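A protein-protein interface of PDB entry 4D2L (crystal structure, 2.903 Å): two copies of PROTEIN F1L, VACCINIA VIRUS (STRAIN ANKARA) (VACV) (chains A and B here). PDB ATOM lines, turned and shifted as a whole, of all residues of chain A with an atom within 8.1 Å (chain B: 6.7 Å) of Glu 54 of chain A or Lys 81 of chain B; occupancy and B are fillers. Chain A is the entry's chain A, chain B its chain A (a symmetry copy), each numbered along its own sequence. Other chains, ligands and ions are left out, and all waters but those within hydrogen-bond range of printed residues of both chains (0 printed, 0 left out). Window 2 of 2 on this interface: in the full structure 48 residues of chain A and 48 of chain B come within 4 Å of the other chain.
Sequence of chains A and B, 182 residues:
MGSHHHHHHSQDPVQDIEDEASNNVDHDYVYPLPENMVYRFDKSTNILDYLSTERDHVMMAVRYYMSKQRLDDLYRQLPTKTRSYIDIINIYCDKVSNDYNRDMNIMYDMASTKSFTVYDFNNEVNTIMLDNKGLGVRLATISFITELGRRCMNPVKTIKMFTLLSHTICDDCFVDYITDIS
The side-chain amino group (NZ) of Lys 81 of chain B lies within salt-bridge range of the side-chain carboxylate (OE2) of Glu 54 of chain A (2.9 Å). The side-chain carboxylate of Glu 54 of chain A sits at hydrogen-bond distance from the side-chain hydroxyl of Tyr 85 of chain B (2.9 Å). A ring nitrogen (ND1) of His 57 of chain A lies within hydrogen-bond range of the side-chain hydroxyl (OG1) of Thr 82 of chain B (2.7 Å).
A ring nitrogen (NE2) of His 57 of chain A is in hydrogen-bond range of the backbone carbonyl oxygen (O) of Leu 51 of chain A (3.1 Å). The backbone carbonyl oxygen of Leu 78 of chain B sits at hydrogen-bond distance from the guanidinium group of Arg 83 of chain B (2.9 Å). OG of Ser 84 of chain B is in hydrogen-bond range of O of Lys 81 of chain B. O of Val 175 of chain B sits close to OG1 of Thr 179 of chain B (3.3 Å).
Leu 78 of chain B touches Leu 51 of chain A (CD2 to CD1, 3.9 Å). Pro 79 of chain B touches Leu 51 of chain A. CD2 of Leu 51 of chain A touches OG1 of Thr 82 of chain B, 3.5 Å away. CG2 of Thr 179 of chain B touches OE1 of Glu 54 of chain A (3.4 Å). CG2 of Val 175 of chain B touches CA of Arg 55 of chain A, 3.8 Å away. His 57 of chain A touches Tyr 85 of chain B. Val 58 of chain A touches Tyr 85 of chain B (N to CD2, 3.9 Å). Met 60 of chain A touches Thr 82 of chain B (CG to CG2, 3.8 Å). CB of Ala 61 of chain A touches CB of Tyr 85 of chain B, at 3.7 Å. Ala 61 of chain A touches Ile 86 of chain B.
Thr 53 of chain A touches none of the printed residues of chain B. Of chain B, only Lys 81, Tyr 85 and Thr 179 come within 4 Å of Glu 54 of chain A. Of the printed residues of chain B, His 57 of chain A touches Lys 81 (3.8 Å), Thr 82 (2.7 Å) and Tyr 85 (3.6 Å). Of the printed residues of chain A, Pro 79 of chain B touches Leu 51 (3.6 Å). Of chain A, only Glu 54 (2.9 Å) and His 57 (3.8 Å) come within 4 Å of Lys 81 of chain B.
Hydrophobic or aromatic side chains of chain A that line the printed part of chain B: Leu 51, His 57, Val 58, Met 60 and Ala 61. Hydrophobic or aromatic side chains of chain B within 4 Å of the printed part of chain A: Leu 78, Pro 79, Tyr 85, Ile 86 and Val 175. Among the printed residues, 14 pairs touch across the chains.
No position is printed for both chains.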
ATOM      1  N   LEU A  51      16.415  17.116 -17.195  1.00  0.00           N
ATOM      2  CA  LEU A  51      15.026  17.124 -17.640  1.00  0.00           C
ATOM      3  C   LEU A  51      14.914  17.076 -19.182  1.00  0.00           C
ATOM      4  O   LEU A  51      14.301  17.960 -19.792  1.00  0.00           O
ATOM      5  CB  LEU A  51      14.306  18.364 -17.090  1.00  0.00           C
ATOM      6  CG  LEU A  51      13.950  18.308 -15.599  1.00  0.00           C
ATOM      7  CD1 LEU A  51      14.030  19.675 -14.930  1.00  0.00           C
ATOM      8  CD2 LEU A  51      12.574  17.710 -15.398  1.00  0.00           C
ATOM      9  N   SER A  52      15.513  16.055 -19.802  1.00  0.00           N
ATOM     10  CA  SER A  52      15.600  15.962 -21.265  1.00  0.00           C
ATOM     11  C   SER A  52      14.239  15.739 -21.920  1.00  0.00           C
ATOM     12  O   SER A  52      13.701  16.626 -22.590  1.00  0.00           O
ATOM     13  CB  SER A  52      16.534  14.819 -21.687  1.00  0.00           C
ATOM     14  OG  SER A  52      17.579  14.613 -20.754  1.00  0.00           O
ATOM     15  N   THR A  53      13.700  14.536 -21.727  1.00  0.00           N
ATOM     16  CA  THR A  53      12.463  14.117 -22.381  1.00  0.00           C
ATOM     17  C   THR A  53      11.218  14.445 -21.552  1.00  0.00           C
ATOM     18  O   THR A  53      11.317  14.917 -20.420  1.00  0.00           O
ATOM     19  CB  THR A  53      12.479  12.598 -22.691  1.00  0.00           C
ATOM     20  OG1 THR A  53      12.575  11.842 -21.475  1.00  0.00           O
ATOM     21  CG2 THR A  53      13.649  12.249 -23.588  1.00  0.00           C
ATOM     22  N   GLU A  54      10.044  14.206 -22.136  1.00  0.00           N
ATOM     23  CA  GLU A  54       8.770  14.413 -21.455  1.00  0.00           C
ATOM     24  C   GLU A  54       8.644  13.502 -20.238  1.00  0.00           C
ATOM     25  O   GLU A  54       8.211  13.934 -19.162  1.00  0.00           O
ATOM     26  CB  GLU A  54       7.599  14.162 -22.409  1.00  0.00           C
ATOM     27  CG  GLU A  54       7.336  15.264 -23.416  1.00  0.00           C
ATOM     28  CD  GLU A  54       6.607  16.462 -22.828  1.00  0.00           C
ATOM     29  OE1 GLU A  54       6.401  16.500 -21.596  1.00  0.00           O
ATOM     30  OE2 GLU A  54       6.222  17.362 -23.606  1.00  0.00           O
ATOM     31  N   ARG A  55       9.014  12.239 -20.423  1.00  0.00           N
ATOM     32  CA  ARG A  55       8.998  11.271 -19.336  1.00  0.00           C
ATOM     33  C   ARG A  55       9.760  11.779 -18.116  1.00  0.00           C
ATOM     34  O   ARG A  55       9.305  11.628 -16.981  1.00  0.00           O
ATOM     35  CB  ARG A  55       9.584   9.945 -19.804  1.00  0.00           C
ATOM     36  CG  ARG A  55       9.747   8.936 -18.713  1.00  0.00           C
ATOM     37  CD  ARG A  55       9.991   7.577 -19.302  1.00  0.00           C
ATOM     38  NE  ARG A  55       9.961   6.550 -18.267  1.00  0.00           N
ATOM     39  CZ  ARG A  55      11.037   5.941 -17.787  1.00  0.00           C
ATOM     40  NH1 ARG A  55      12.234   6.243 -18.256  1.00  0.00           N
ATOM     41  NH2 ARG A  55      10.914   5.030 -16.841  1.00  0.00           N
ATOM     42  N   ASP A  56      10.906  12.404 -18.360  1.00  0.00           N
ATOM     43  CA  ASP A  56      11.751  12.908 -17.281  1.00  0.00           C
ATOM     44  C   ASP A  56      11.079  13.994 -16.451  1.00  0.00           C
ATOM     45  O   ASP A  56      11.300  14.078 -15.240  1.00  0.00           O
ATOM     46  CB  ASP A  56      13.064  13.427 -17.855  1.00  0.00           C
ATOM     47  CG  ASP A  56      13.830  12.351 -18.582  1.00  0.00           C
ATOM     48  OD1 ASP A  56      13.198  11.361 -19.022  1.00  0.00           O
ATOM     49  OD2 ASP A  56      15.061  12.496 -18.714  1.00  0.00           O
ATOM     50  N   HIS A  57      10.266  14.818 -17.104  1.00  0.00           N
ATOM     51  CA  HIS A  57       9.469  15.820 -16.408  1.00  0.00           C
ATOM     52  C   HIS A  57       8.391  15.197 -15.537  1.00  0.00           C
ATOM     53  O   HIS A  57       8.228  15.585 -14.384  1.00  0.00           O
ATOM     54  CB  HIS A  57       8.824  16.769 -17.409  1.00  0.00           C
ATOM     55  CG  HIS A  57       9.793  17.675 -18.075  1.00  0.00           C
ATOM     56  ND1 HIS A  57      10.144  18.904 -17.557  1.00  0.00           N
ATOM     57  CD2 HIS A  57      10.517  17.527 -19.214  1.00  0.00           C
ATOM     58  CE1 HIS A  57      11.031  19.473 -18.350  1.00  0.00           C
ATOM     59  NE2 HIS A  57      11.273  18.667 -19.356  1.00  0.00           N
ATOM     60  N   VAL A  58       7.641  14.250 -16.091  1.00  0.00           N
ATOM     61  CA  VAL A  58       6.593  13.601 -15.323  1.00  0.00           C
ATOM     62  C   VAL A  58       7.181  12.793 -14.167  1.00  0.00           C
ATOM     63  O   VAL A  58       6.667  12.821 -13.046  1.00  0.00           O
ATOM     64  CB  VAL A  58       5.733  12.684 -16.202  1.00  0.00           C
ATOM     65  CG1 VAL A  58       4.602  12.123 -15.394  1.00  0.00           C
ATOM     66  CG2 VAL A  58       5.176  13.459 -17.385  1.00  0.00           C
ATOM     67  N   MET A  59       8.271  12.091 -14.455  1.00  0.00           N
ATOM     68  CA  MET A  59       8.963  11.261 -13.474  1.00  0.00           C
ATOM     69  C   MET A  59       9.504  12.103 -12.309  1.00  0.00           C
ATOM     70  O   MET A  59       9.540  11.675 -11.162  1.00  0.00           O
ATOM     71  CB  MET A  59      10.086  10.492 -14.169  1.00  0.00           C
ATOM     72  CG  MET A  59      10.753   9.412 -13.349  1.00  0.00           C
ATOM     73  SD  MET A  59      11.369   8.056 -14.378  1.00  0.00           S
ATOM     74  CE  MET A  59      12.338   8.934 -15.599  1.00  0.00           C
ATOM     75  N   MET A  60       9.914  13.317 -12.623  1.00  0.00           N
ATOM     76  CA  MET A  60      10.431  14.245 -11.635  1.00  0.00           C
ATOM     77  C   MET A  60       9.268  14.745 -10.781  1.00  0.00           C
ATOM     78  O   MET A  60       9.363  14.793  -9.556  1.00  0.00           O
ATOM     79  CB  MET A  60      11.178  15.397 -12.339  1.00  0.00           C
ATOM     80  CG  MET A  60      11.658  16.556 -11.464  1.00  0.00           C
ATOM     81  SD  MET A  60      12.822  16.090 -10.175  1.00  0.00           S
ATOM     82  CE  MET A  60      13.968  15.099 -11.115  1.00  0.00           C
ATOM     83  N   ALA A  61       8.171  15.102 -11.438  1.00  0.00           N
ATOM     84  CA  ALA A  61       7.008  15.613 -10.743  1.00  0.00           C
ATOM     85  C   ALA A  61       6.464  14.555  -9.775  1.00  0.00           C
ATOM     86  O   ALA A  61       6.210  14.860  -8.613  1.00  0.00           O
ATOM     87  CB  ALA A  61       5.951  16.044 -11.735  1.00  0.00           C
ATOM     88  N   LEU B  78      13.144  24.533 -10.770  1.00  0.00           N
ATOM     89  CA  LEU B  78      12.413  23.710 -11.732  1.00  0.00           C
ATOM     90  C   LEU B  78      11.723  24.554 -12.794  1.00  0.00           C
ATOM     91  O   LEU B  78      11.165  25.611 -12.488  1.00  0.00           O
ATOM     92  CB  LEU B  78      11.364  22.837 -11.028  1.00  0.00           C
ATOM     93  CG  LEU B  78      11.798  21.484 -10.477  1.00  0.00           C
ATOM     94  CD1 LEU B  78      10.633  20.819  -9.775  1.00  0.00           C
ATOM     95  CD2 LEU B  78      12.308  20.607 -11.598  1.00  0.00           C
ATOM     96  N   PRO B  79      11.751  24.080 -14.049  1.00  0.00           N
ATOM     97  CA  PRO B  79      11.028  24.738 -15.148  1.00  0.00           C
ATOM     98  C   PRO B  79       9.524  24.755 -14.910  1.00  0.00           C
ATOM     99  O   PRO B  79       8.994  23.912 -14.183  1.00  0.00           O
ATOM    100  CB  PRO B  79      11.385  23.892 -16.382  1.00  0.00           C
ATOM    101  CG  PRO B  79      12.010  22.637 -15.853  1.00  0.00           C
ATOM    102  CD  PRO B  79      12.601  22.971 -14.518  1.00  0.00           C
ATOM    103  N   THR B  80       8.844  25.719 -15.515  1.00  0.00           N
ATOM    104  CA  THR B  80       7.418  25.880 -15.288  1.00  0.00           C
ATOM    105  C   THR B  80       6.627  24.676 -15.806  1.00  0.00           C
ATOM    106  O   THR B  80       5.512  24.415 -15.346  1.00  0.00           O
ATOM    107  CB  THR B  80       6.905  27.166 -15.944  1.00  0.00           C
ATOM    108  OG1 THR B  80       7.608  27.374 -17.173  1.00  0.00           O
ATOM    109  CG2 THR B  80       7.157  28.353 -15.024  1.00  0.00           C
ATOM    110  N   LYS B  81       7.219  23.944 -16.752  1.00  0.00           N
ATOM    111  CA  LYS B  81       6.607  22.737 -17.309  1.00  0.00           C
ATOM    112  C   LYS B  81       6.484  21.662 -16.241  1.00  0.00           C
ATOM    113  O   LYS B  81       5.396  21.178 -15.940  1.00  0.00           O
ATOM    114  CB  LYS B  81       7.434  22.209 -18.478  1.00  0.00           C
ATOM    115  CG  LYS B  81       6.872  20.964 -19.128  1.00  0.00           C
ATOM    116  CD  LYS B  81       7.824  20.433 -20.178  1.00  0.00           C
ATOM    117  CE  LYS B  81       7.076  19.683 -21.263  1.00  0.00           C
ATOM    118  NZ  LYS B  81       7.980  19.301 -22.382  1.00  0.00           N
ATOM    119  N   THR B  82       7.630  21.300 -15.680  1.00  0.00           N
ATOM    120  CA  THR B  82       7.709  20.390 -14.553  1.00  0.00           C
ATOM    121  C   THR B  82       6.805  20.869 -13.421  1.00  0.00           C
ATOM    122  O   THR B  82       6.090  20.082 -12.808  1.00  0.00           O
ATOM    123  CB  THR B  82       9.159  20.286 -14.033  1.00  0.00           C
ATOM    124  OG1 THR B  82      10.066  20.197 -15.140  1.00  0.00           O
ATOM    125  CG2 THR B  82       9.322  19.057 -13.155  1.00  0.00           C
ATOM    126  N   ARG B  83       6.847  22.170 -13.152  1.00  0.00           N
ATOM    127  CA  ARG B  83       6.098  22.755 -12.048  1.00  0.00           C
ATOM    128  C   ARG B  83       4.612  22.504 -12.196  1.00  0.00           C
ATOM    129  O   ARG B  83       3.908  22.302 -11.212  1.00  0.00           O
ATOM    130  CB  ARG B  83       6.339  24.258 -11.962  1.00  0.00           C
ATOM    131  CG  ARG B  83       7.621  24.681 -11.295  1.00  0.00           C
ATOM    132  CD  ARG B  83       7.720  26.182 -11.411  1.00  0.00           C
ATOM    133  NE  ARG B  83       8.974  26.727 -10.902  1.00  0.00           N
ATOM    134  CZ  ARG B  83       9.051  27.646  -9.944  1.00  0.00           C
ATOM    135  NH1 ARG B  83       7.936  28.123  -9.391  1.00  0.00           N
ATOM    136  NH2 ARG B  83      10.240  28.101  -9.550  1.00  0.00           N
ATOM    137  N   SER B  84       4.145  22.537 -13.438  1.00  0.00           N
ATOM    138  CA  SER B  84       2.730  22.373 -13.736  1.00  0.00           C
ATOM    139  C   SER B  84       2.326  20.910 -13.652  1.00  0.00           C
ATOM    140  O   SER B  84       1.200  20.591 -13.257  1.00  0.00           O
ATOM    141  CB  SER B  84       2.409  22.904 -15.127  1.00  0.00           C
ATOM    142  OG  SER B  84       2.736  21.923 -16.097  1.00  0.00           O
ATOM    143  N   TYR B  85       3.238  20.028 -14.061  1.00  0.00           N
ATOM    144  CA  TYR B  85       3.023  18.594 -13.935  1.00  0.00           C
ATOM    145  C   TYR B  85       2.843  18.283 -12.470  1.00  0.00           C
ATOM    146  O   TYR B  85       1.882  17.609 -12.086  1.00  0.00           O
ATOM    147  CB  TYR B  85       4.186  17.794 -14.522  1.00  0.00           C
ATOM    148  CG  TYR B  85       4.250  17.851 -16.027  1.00  0.00           C
ATOM    149  CD1 TYR B  85       3.207  18.406 -16.761  1.00  0.00           C
ATOM    150  CD2 TYR B  85       5.346  17.351 -16.715  1.00  0.00           C
ATOM    151  CE1 TYR B  85       3.253  18.468 -18.137  1.00  0.00           C
ATOM    152  CE2 TYR B  85       5.401  17.408 -18.105  1.00  0.00           C
ATOM    153  CZ  TYR B  85       4.347  17.969 -18.806  1.00  0.00           C
ATOM    154  OH  TYR B  85       4.376  18.035 -20.176  1.00  0.00           O
ATOM    155  N   ILE B  86       3.765  18.799 -11.658  1.00  0.00           N
ATOM    156  CA  ILE B  86       3.658  18.713 -10.207  1.00  0.00           C
ATOM    157  C   ILE B  86       2.281  19.170  -9.711  1.00  0.00           C
ATOM    158  O   ILE B  86       1.726  18.580  -8.796  1.00  0.00           O
ATOM    159  CB  ILE B  86       4.739  19.553  -9.518  1.00  0.00           C
ATOM    160  CG1 ILE B  86       6.120  18.965  -9.769  1.00  0.00           C
ATOM    161  CG2 ILE B  86       4.495  19.635  -8.023  1.00  0.00           C
ATOM    162  CD1 ILE B  86       7.217  19.764  -9.129  1.00  0.00           C
ATOM    163  N   VAL B 175       2.785   8.984 -19.084  1.00  0.00           N
ATOM    164  CA  VAL B 175       3.342  10.229 -19.588  1.00  0.00           C
ATOM    165  C   VAL B 175       2.385  10.898 -20.575  1.00  0.00           C
ATOM    166  O   VAL B 175       2.143  12.104 -20.498  1.00  0.00           O
ATOM    167  CB  VAL B 175       4.699   9.997 -20.267  1.00  0.00           C
ATOM    168  CG1 VAL B 175       5.206  11.284 -20.884  1.00  0.00           C
ATOM    169  CG2 VAL B 175       5.709   9.447 -19.265  1.00  0.00           C
ATOM    170  N   THR B 179       0.873  14.827 -19.921  1.00  0.00           N
ATOM    171  CA  THR B 179       1.245  15.930 -20.800  1.00  0.00           C
ATOM    172  C   THR B 179       0.026  16.581 -21.439  1.00  0.00           C
ATOM    173  O   THR B 179       0.047  17.773 -21.756  1.00  0.00           O
ATOM    174  CB  THR B 179       2.206  15.465 -21.902  1.00  0.00           C
ATOM    175  OG1 THR B 179       1.565  14.480 -22.716  1.00  0.00           O
ATOM    176  CG2 THR B 179       3.470  14.878 -21.293  1.00  0.00           C
